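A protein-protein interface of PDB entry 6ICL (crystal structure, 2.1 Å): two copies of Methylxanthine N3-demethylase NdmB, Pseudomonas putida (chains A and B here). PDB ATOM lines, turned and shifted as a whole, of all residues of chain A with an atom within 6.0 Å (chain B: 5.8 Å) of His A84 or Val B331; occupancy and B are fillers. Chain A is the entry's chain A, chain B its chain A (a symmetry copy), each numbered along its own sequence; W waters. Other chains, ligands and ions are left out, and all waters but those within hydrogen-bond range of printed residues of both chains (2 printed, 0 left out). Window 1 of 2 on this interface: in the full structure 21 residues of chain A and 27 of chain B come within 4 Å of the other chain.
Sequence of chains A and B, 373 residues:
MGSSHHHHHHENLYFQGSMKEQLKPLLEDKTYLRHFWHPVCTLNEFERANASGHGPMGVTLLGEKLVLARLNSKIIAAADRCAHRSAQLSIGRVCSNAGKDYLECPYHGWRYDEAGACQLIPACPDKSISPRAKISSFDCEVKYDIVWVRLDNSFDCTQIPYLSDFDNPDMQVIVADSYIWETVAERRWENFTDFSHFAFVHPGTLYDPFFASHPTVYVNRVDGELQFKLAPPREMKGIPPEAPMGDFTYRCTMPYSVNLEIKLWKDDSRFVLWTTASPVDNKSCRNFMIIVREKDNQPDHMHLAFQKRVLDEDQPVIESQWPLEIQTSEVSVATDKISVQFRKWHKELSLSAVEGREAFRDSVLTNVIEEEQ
O of Ala A83 lies within hydrogen-bond range of N of Val B331.
The backbone NH (N) of Val B331 is in hydrogen-bond range of the backbone carbonyl oxygen (O) of His A84, 3.4 Å away.
A ring nitrogen (NE2) of His A84 lies within hydrogen-bond range of the side-chain carboxylate (OD2) of Asp B336 (2.7 Å).
The guanidinium group of Arg A85 sits at hydrogen-bond distance from the side-chain hydroxyl of Ser B332.
The side-chain carboxylate (OD2) of Asp B336 lies within salt-bridge range of the guanidinium group (NH2) of Arg A85, 3.8 Å away.
The side-chain hydroxyl (OG) of Ser A86 lies within hydrogen-bond range of the side-chain carboxylate (OE1) of Glu B330, at 3.5 Å.
The backbone carbonyl oxygen (O) of Ser B329 is in hydrogen-bond range of the guanidinium group (NH2) of Arg A132 (3.5 Å).
NH1 of Arg A132 lies within hydrogen-bond range of O of Glu B330 (3.1 Å).
SG of Cys A82 lies close to N of His A84 (3.5 Å).
N of Ala A83 sits at hydrogen-bond distance from OH of Tyr A112, at 3.1 Å.
The side-chain hydroxyl (OG) of Ser A130 is in hydrogen-bond range of the backbone NH (N) of Arg A132 (2.9 Å).
The backbone NH (N) of Val B333 is in hydrogen-bond range of the side-chain carboxylate (OD2) of Asp B336 (2.9 Å).
Among the printed residues, merely in contact across the chains: His A108 with Ser B196, His A84 with Glu B330, Arg A85 with Glu B330, Arg A85 with Val B331, Arg A132 with Val B331, Trp A110 with Val B333, Trp A110 with Val B331 and Ala A83 with Glu B330.
His A84 touches three residues of chain B.
Val B331 touches just these residues of chain A: Ala A83, His A84, Arg A85, Trp A110 and Arg A132.
Printed residues of chain A within 4 Å of Asp B336: His A84 and Arg A85.
Printed residues of chain B within 4 Å of Ala A83: Glu B330 (3.8 Å) and Val B331 (2.9 Å).
Printed residues of chain A within 4 Å of Val B333: Trp A110.
Of the printed residues of chain B, Trp A110 touches Val B331 (3.7 Å) and Val B333 (3.7 Å).
Of the printed residues of chain B, Arg A85 touches Glu B330 (3.4 Å), Val B331 (3.6 Å), Ser B332 (2.9 Å) and Asp B336 (3.5 Å).
Cys A82 touches none of the printed residues of chain B.
The nearest printed residue of chain B that does not touch His A84 is Val B333 (4.6 Å).
Hydrophobic or aromatic side chains of chain A within 4 Å of the printed part of chain B: His A84, His A108 and Trp A110.
Among the printed residues, Asp or Glu carboxylates within 4 Å of a Lys or Arg side-chain nitrogen of the other chain: Arg A85 with Asp B336.
No position is printed for both chains.
Of the 16 pairs that touch across the chains among the printed residues, none has its exchanged pair printed and touching as well.
Water W2 lies within hydrogen-bond range of NH1 of Arg A132 (2.9 Å) and N of Ser B332 (2.9 Å).
Water W1 lies within hydrogen-bond range of O of Ser B329 (3.1 Å) and O of Ala A83 (3.4 Å).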
ATOM      1  N   CYS A  82     -14.188   7.871  17.223  1.00  0.00           N
ATOM      2  CA  CYS A  82     -13.512   9.123  17.521  1.00  0.00           C
ATOM      3  C   CYS A  82     -12.372   9.343  16.538  1.00  0.00           C
ATOM      4  O   CYS A  82     -11.676   8.405  16.151  1.00  0.00           O
ATOM      5  CB  CYS A  82     -12.986   9.110  18.950  1.00  0.00           C
ATOM      6  SG  CYS A  82     -12.185  10.651  19.429  1.00  0.00           S
ATOM      7  N   ALA A  83     -12.189  10.599  16.119  1.00  0.00           N
ATOM      8  CA  ALA A  83     -11.133  10.909  15.155  1.00  0.00           C
ATOM      9  C   ALA A  83      -9.744  10.821  15.767  1.00  0.00           C
ATOM     10  O   ALA A  83      -8.762  10.667  15.030  1.00  0.00           O
ATOM     11  CB  ALA A  83     -11.340  12.315  14.566  1.00  0.00           C
ATOM     12  N   HIS A  84      -9.634  10.930  17.090  1.00  0.00           N
ATOM     13  CA  HIS A  84      -8.322  10.908  17.722  1.00  0.00           C
ATOM     14  C   HIS A  84      -7.697   9.517  17.658  1.00  0.00           C
ATOM     15  O   HIS A  84      -6.698   9.309  16.955  1.00  0.00           O
ATOM     16  CB  HIS A  84      -8.414  11.380  19.179  1.00  0.00           C
ATOM     17  CG  HIS A  84      -7.102  11.363  19.895  1.00  0.00           C
ATOM     18  ND1 HIS A  84      -6.975  11.000  21.217  1.00  0.00           N
ATOM     19  CD2 HIS A  84      -5.851  11.647  19.466  1.00  0.00           C
ATOM     20  CE1 HIS A  84      -5.710  11.075  21.581  1.00  0.00           C
ATOM     21  NE2 HIS A  84      -5.005  11.468  20.536  1.00  0.00           N
ATOM     22  N   ARG A  85      -8.267   8.557  18.406  1.00  0.00           N
ATOM     23  CA  ARG A  85      -7.700   7.211  18.427  1.00  0.00           C
ATOM     24  C   ARG A  85      -8.757   6.122  18.253  1.00  0.00           C
ATOM     25  O   ARG A  85      -8.540   4.979  18.698  1.00  0.00           O
ATOM     26  CB  ARG A  85      -6.898   6.959  19.722  1.00  0.00           C
ATOM     27  CG  ARG A  85      -5.565   7.747  19.834  1.00  0.00           C
ATOM     28  CD  ARG A  85      -4.588   7.308  18.749  1.00  0.00           C
ATOM     29  NE  ARG A  85      -3.234   7.868  18.899  1.00  0.00           N
ATOM     30  CZ  ARG A  85      -2.741   8.857  18.154  1.00  0.00           C
ATOM     31  NH1 ARG A  85      -3.489   9.414  17.202  1.00  0.00           N
ATOM     32  NH2 ARG A  85      -1.499   9.288  18.358  1.00  0.00           N
ATOM     33  N   SER A  86      -9.891   6.447  17.636  1.00  0.00           N
ATOM     34  CA  SER A  86     -10.858   5.500  17.102  1.00  0.00           C
ATOM     35  C   SER A  86     -11.699   4.810  18.165  1.00  0.00           C
ATOM     36  O   SER A  86     -12.345   3.809  17.832  1.00  0.00           O
ATOM     37  CB  SER A  86     -10.198   4.400  16.258  1.00  0.00           C
ATOM     38  OG  SER A  86      -9.429   4.951  15.206  1.00  0.00           O
ATOM     39  N   HIS A 108      -9.966   9.841  25.571  1.00  0.00           N
ATOM     40  CA  HIS A 108      -9.245  11.044  26.000  1.00  0.00           C
ATOM     41  C   HIS A 108     -10.136  12.289  26.014  1.00  0.00           C
ATOM     42  O   HIS A 108      -9.626  13.404  26.044  1.00  0.00           O
ATOM     43  CB  HIS A 108      -8.003  11.293  25.139  1.00  0.00           C
ATOM     44  CG  HIS A 108      -7.126  10.085  24.958  1.00  0.00           C
ATOM     45  ND1 HIS A 108      -7.333   9.156  23.962  1.00  0.00           N
ATOM     46  CD2 HIS A 108      -6.011   9.683  25.617  1.00  0.00           C
ATOM     47  CE1 HIS A 108      -6.399   8.218  24.028  1.00  0.00           C
ATOM     48  NE2 HIS A 108      -5.590   8.513  25.029  1.00  0.00           N
ATOM     49  N   TRP A 110     -12.295  13.997  23.982  1.00  0.00           N
ATOM     50  CA  TRP A 110     -12.636  14.969  22.953  1.00  0.00           C
ATOM     51  C   TRP A 110     -14.145  15.135  22.924  1.00  0.00           C
ATOM     52  O   TRP A 110     -14.898  14.181  23.147  1.00  0.00           O
ATOM     53  CB  TRP A 110     -12.110  14.539  21.581  1.00  0.00           C
ATOM     54  CG  TRP A 110     -10.601  14.564  21.442  1.00  0.00           C
ATOM     55  CD1 TRP A 110      -9.680  14.563  22.445  1.00  0.00           C
ATOM     56  CD2 TRP A 110      -9.850  14.601  20.211  1.00  0.00           C
ATOM     57  NE1 TRP A 110      -8.395  14.590  21.916  1.00  0.00           N
ATOM     58  CE2 TRP A 110      -8.479  14.616  20.551  1.00  0.00           C
ATOM     59  CE3 TRP A 110     -10.208  14.627  18.856  1.00  0.00           C
ATOM     60  CZ2 TRP A 110      -7.461  14.655  19.584  1.00  0.00           C
ATOM     61  CZ3 TRP A 110      -9.195  14.662  17.895  1.00  0.00           C
ATOM     62  CH2 TRP A 110      -7.842  14.669  18.269  1.00  0.00           C
ATOM     63  N   TYR A 112     -17.583  16.451  20.911  1.00  0.00           N
ATOM     64  CA  TYR A 112     -18.146  16.696  19.595  1.00  0.00           C
ATOM     65  C   TYR A 112     -19.491  17.402  19.731  1.00  0.00           C
ATOM     66  O   TYR A 112     -20.268  17.115  20.652  1.00  0.00           O
ATOM     67  CB  TYR A 112     -18.285  15.388  18.807  1.00  0.00           C
ATOM     68  CG  TYR A 112     -16.954  14.767  18.465  1.00  0.00           C
ATOM     69  CD1 TYR A 112     -16.304  15.076  17.273  1.00  0.00           C
ATOM     70  CD2 TYR A 112     -16.328  13.889  19.351  1.00  0.00           C
ATOM     71  CE1 TYR A 112     -15.056  14.514  16.970  1.00  0.00           C
ATOM     72  CE2 TYR A 112     -15.101  13.326  19.056  1.00  0.00           C
ATOM     73  CZ  TYR A 112     -14.478  13.629  17.868  1.00  0.00           C
ATOM     74  OH  TYR A 112     -13.258  13.055  17.599  1.00  0.00           O
ATOM     75  N   SER A 130      -7.695  21.447  15.009  1.00  0.00           N
ATOM     76  CA  SER A 130      -7.545  21.101  13.600  1.00  0.00           C
ATOM     77  C   SER A 130      -8.888  20.785  12.945  1.00  0.00           C
ATOM     78  O   SER A 130      -9.780  20.227  13.596  1.00  0.00           O
ATOM     79  CB  SER A 130      -6.606  19.902  13.460  1.00  0.00           C
ATOM     80  OG  SER A 130      -6.868  19.184  12.264  1.00  0.00           O
ATOM     81  N   ARG A 132      -9.203  18.498  10.740  1.00  0.00           N
ATOM     82  CA  ARG A 132      -9.142  17.041  10.684  1.00  0.00           C
ATOM     83  C   ARG A 132      -9.908  16.383  11.834  1.00  0.00           C
ATOM     84  O   ARG A 132     -10.341  15.231  11.699  1.00  0.00           O
ATOM     85  CB  ARG A 132      -7.668  16.606  10.689  1.00  0.00           C
ATOM     86  CG  ARG A 132      -7.266  15.660   9.565  1.00  0.00           C
ATOM     87  CD  ARG A 132      -5.757  15.688   9.261  1.00  0.00           C
ATOM     88  NE  ARG A 132      -4.931  14.834  10.129  1.00  0.00           N
ATOM     89  CZ  ARG A 132      -4.902  13.498  10.098  1.00  0.00           C
ATOM     90  NH1 ARG A 132      -4.096  12.835  10.921  1.00  0.00           N
ATOM     91  NH2 ARG A 132      -5.680  12.810   9.262  1.00  0.00           N
ATOM     92  N   ALA A 133     -10.097  17.094  12.948  1.00  0.00           N
ATOM     93  CA  ALA A 133     -10.738  16.556  14.147  1.00  0.00           C
ATOM     94  C   ALA A 133     -12.249  16.707  14.009  1.00  0.00           C
ATOM     95  O   ALA A 133     -12.881  17.624  14.541  1.00  0.00           O
ATOM     96  CB  ALA A 133     -10.211  17.255  15.393  1.00  0.00           C
ATOM     97  N   LYS A 134     -12.836  15.776  13.281  1.00  0.00           N
ATOM     98  CA  LYS A 134     -14.225  15.920  12.885  1.00  0.00           C
ATOM     99  C   LYS A 134     -14.716  14.554  12.445  1.00  0.00           C
ATOM    100  O   LYS A 134     -13.968  13.795  11.819  1.00  0.00           O
ATOM    101  CB  LYS A 134     -14.363  16.958  11.767  1.00  0.00           C
ATOM    102  CG  LYS A 134     -15.504  16.725  10.791  1.00  0.00           C
ATOM    103  CD  LYS A 134     -15.694  17.925   9.868  1.00  0.00           C
ATOM    104  CE  LYS A 134     -16.281  19.118  10.625  1.00  0.00           C
ATOM    105  NZ  LYS A 134     -17.587  18.761  11.251  1.00  0.00           N
ATOM    106  N   SER B 196      -3.105  11.169  29.377  1.00  0.00           N
ATOM    107  CA  SER B 196      -4.243  12.042  29.120  1.00  0.00           C
ATOM    108  C   SER B 196      -5.588  11.327  29.212  1.00  0.00           C
ATOM    109  O   SER B 196      -6.616  12.006  29.251  1.00  0.00           O
ATOM    110  CB  SER B 196      -4.099  12.699  27.753  1.00  0.00           C
ATOM    111  OG  SER B 196      -4.130  11.735  26.733  1.00  0.00           O
ATOM    112  N   SER B 329      -5.319   7.450   9.222  1.00  0.00           N
ATOM    113  CA  SER B 329      -6.209   8.595   9.350  1.00  0.00           C
ATOM    114  C   SER B 329      -6.376   9.094  10.784  1.00  0.00           C
ATOM    115  O   SER B 329      -7.036  10.120  10.983  1.00  0.00           O
ATOM    116  CB  SER B 329      -7.588   8.241   8.803  1.00  0.00           C
ATOM    117  OG  SER B 329      -8.303   7.461   9.750  1.00  0.00           O
ATOM    118  N   GLU B 330      -5.840   8.399  11.788  1.00  0.00           N
ATOM    119  CA  GLU B 330      -6.024   8.842  13.166  1.00  0.00           C
ATOM    120  C   GLU B 330      -5.340  10.191  13.389  1.00  0.00           C
ATOM    121  O   GLU B 330      -4.265  10.457  12.851  1.00  0.00           O
ATOM    122  CB  GLU B 330      -5.492   7.788  14.145  1.00  0.00           C
ATOM    123  CG  GLU B 330      -6.463   6.611  14.367  1.00  0.00           C
ATOM    124  CD  GLU B 330      -5.770   5.381  14.972  1.00  0.00           C
ATOM    125  OE1 GLU B 330      -6.088   4.244  14.580  1.00  0.00           O
ATOM    126  OE2 GLU B 330      -4.865   5.551  15.800  1.00  0.00           O
ATOM    127  N   VAL B 331      -5.977  11.054  14.172  1.00  0.00           N
ATOM    128  CA  VAL B 331      -5.548  12.446  14.298  1.00  0.00           C
ATOM    129  C   VAL B 331      -4.730  12.577  15.573  1.00  0.00           C
ATOM    130  O   VAL B 331      -5.271  12.464  16.678  1.00  0.00           O
ATOM    131  CB  VAL B 331      -6.744  13.409  14.313  1.00  0.00           C
ATOM    132  CG1 VAL B 331      -6.264  14.825  14.624  1.00  0.00           C
ATOM    133  CG2 VAL B 331      -7.507  13.355  12.988  1.00  0.00           C
ATOM    134  N   SER B 332      -3.435  12.849  15.437  1.00  0.00           N
ATOM    135  CA  SER B 332      -2.552  13.065  16.581  1.00  0.00           C
ATOM    136  C   SER B 332      -2.389  14.548  16.900  1.00  0.00           C
ATOM    137  O   SER B 332      -2.229  15.379  16.000  1.00  0.00           O
ATOM    138  CB  SER B 332      -1.183  12.443  16.326  1.00  0.00           C
ATOM    139  OG  SER B 332      -1.318  11.053  16.104  1.00  0.00           O
ATOM    140  N   VAL B 333      -2.417  14.868  18.195  1.00  0.00           N
ATOM    141  CA  VAL B 333      -2.168  16.219  18.693  1.00  0.00           C
ATOM    142  C   VAL B 333      -0.857  16.222  19.472  1.00  0.00           C
ATOM    143  O   VAL B 333      -0.182  15.188  19.585  1.00  0.00           O
ATOM    144  CB  VAL B 333      -3.336  16.740  19.560  1.00  0.00           C
ATOM    145  CG1 VAL B 333      -4.591  16.881  18.723  1.00  0.00           C
ATOM    146  CG2 VAL B 333      -3.600  15.818  20.753  1.00  0.00           C
ATOM    147  N   ASP B 336       0.341  13.614  22.020  1.00  0.00           N
ATOM    148  CA  ASP B 336       0.556  12.229  21.605  1.00  0.00           C
ATOM    149  C   ASP B 336       1.996  11.956  21.179  1.00  0.00           C
ATOM    150  O   ASP B 336       2.257  10.951  20.504  1.00  0.00           O
ATOM    151  CB  ASP B 336      -0.392  11.854  20.470  1.00  0.00           C
ATOM    152  CG  ASP B 336      -1.862  12.066  20.824  1.00  0.00           C
ATOM    153  OD1 ASP B 336      -2.283  11.760  21.956  1.00  0.00           O
ATOM    154  OD2 ASP B 336      -2.610  12.543  19.946  1.00  0.00           O
HETATM  155  O   HOH W   1      -9.778   9.128  12.132  1.00  0.00           O
HETATM  156  O   HOH W   2      -2.093  13.379  12.911  1.00  0.00           O
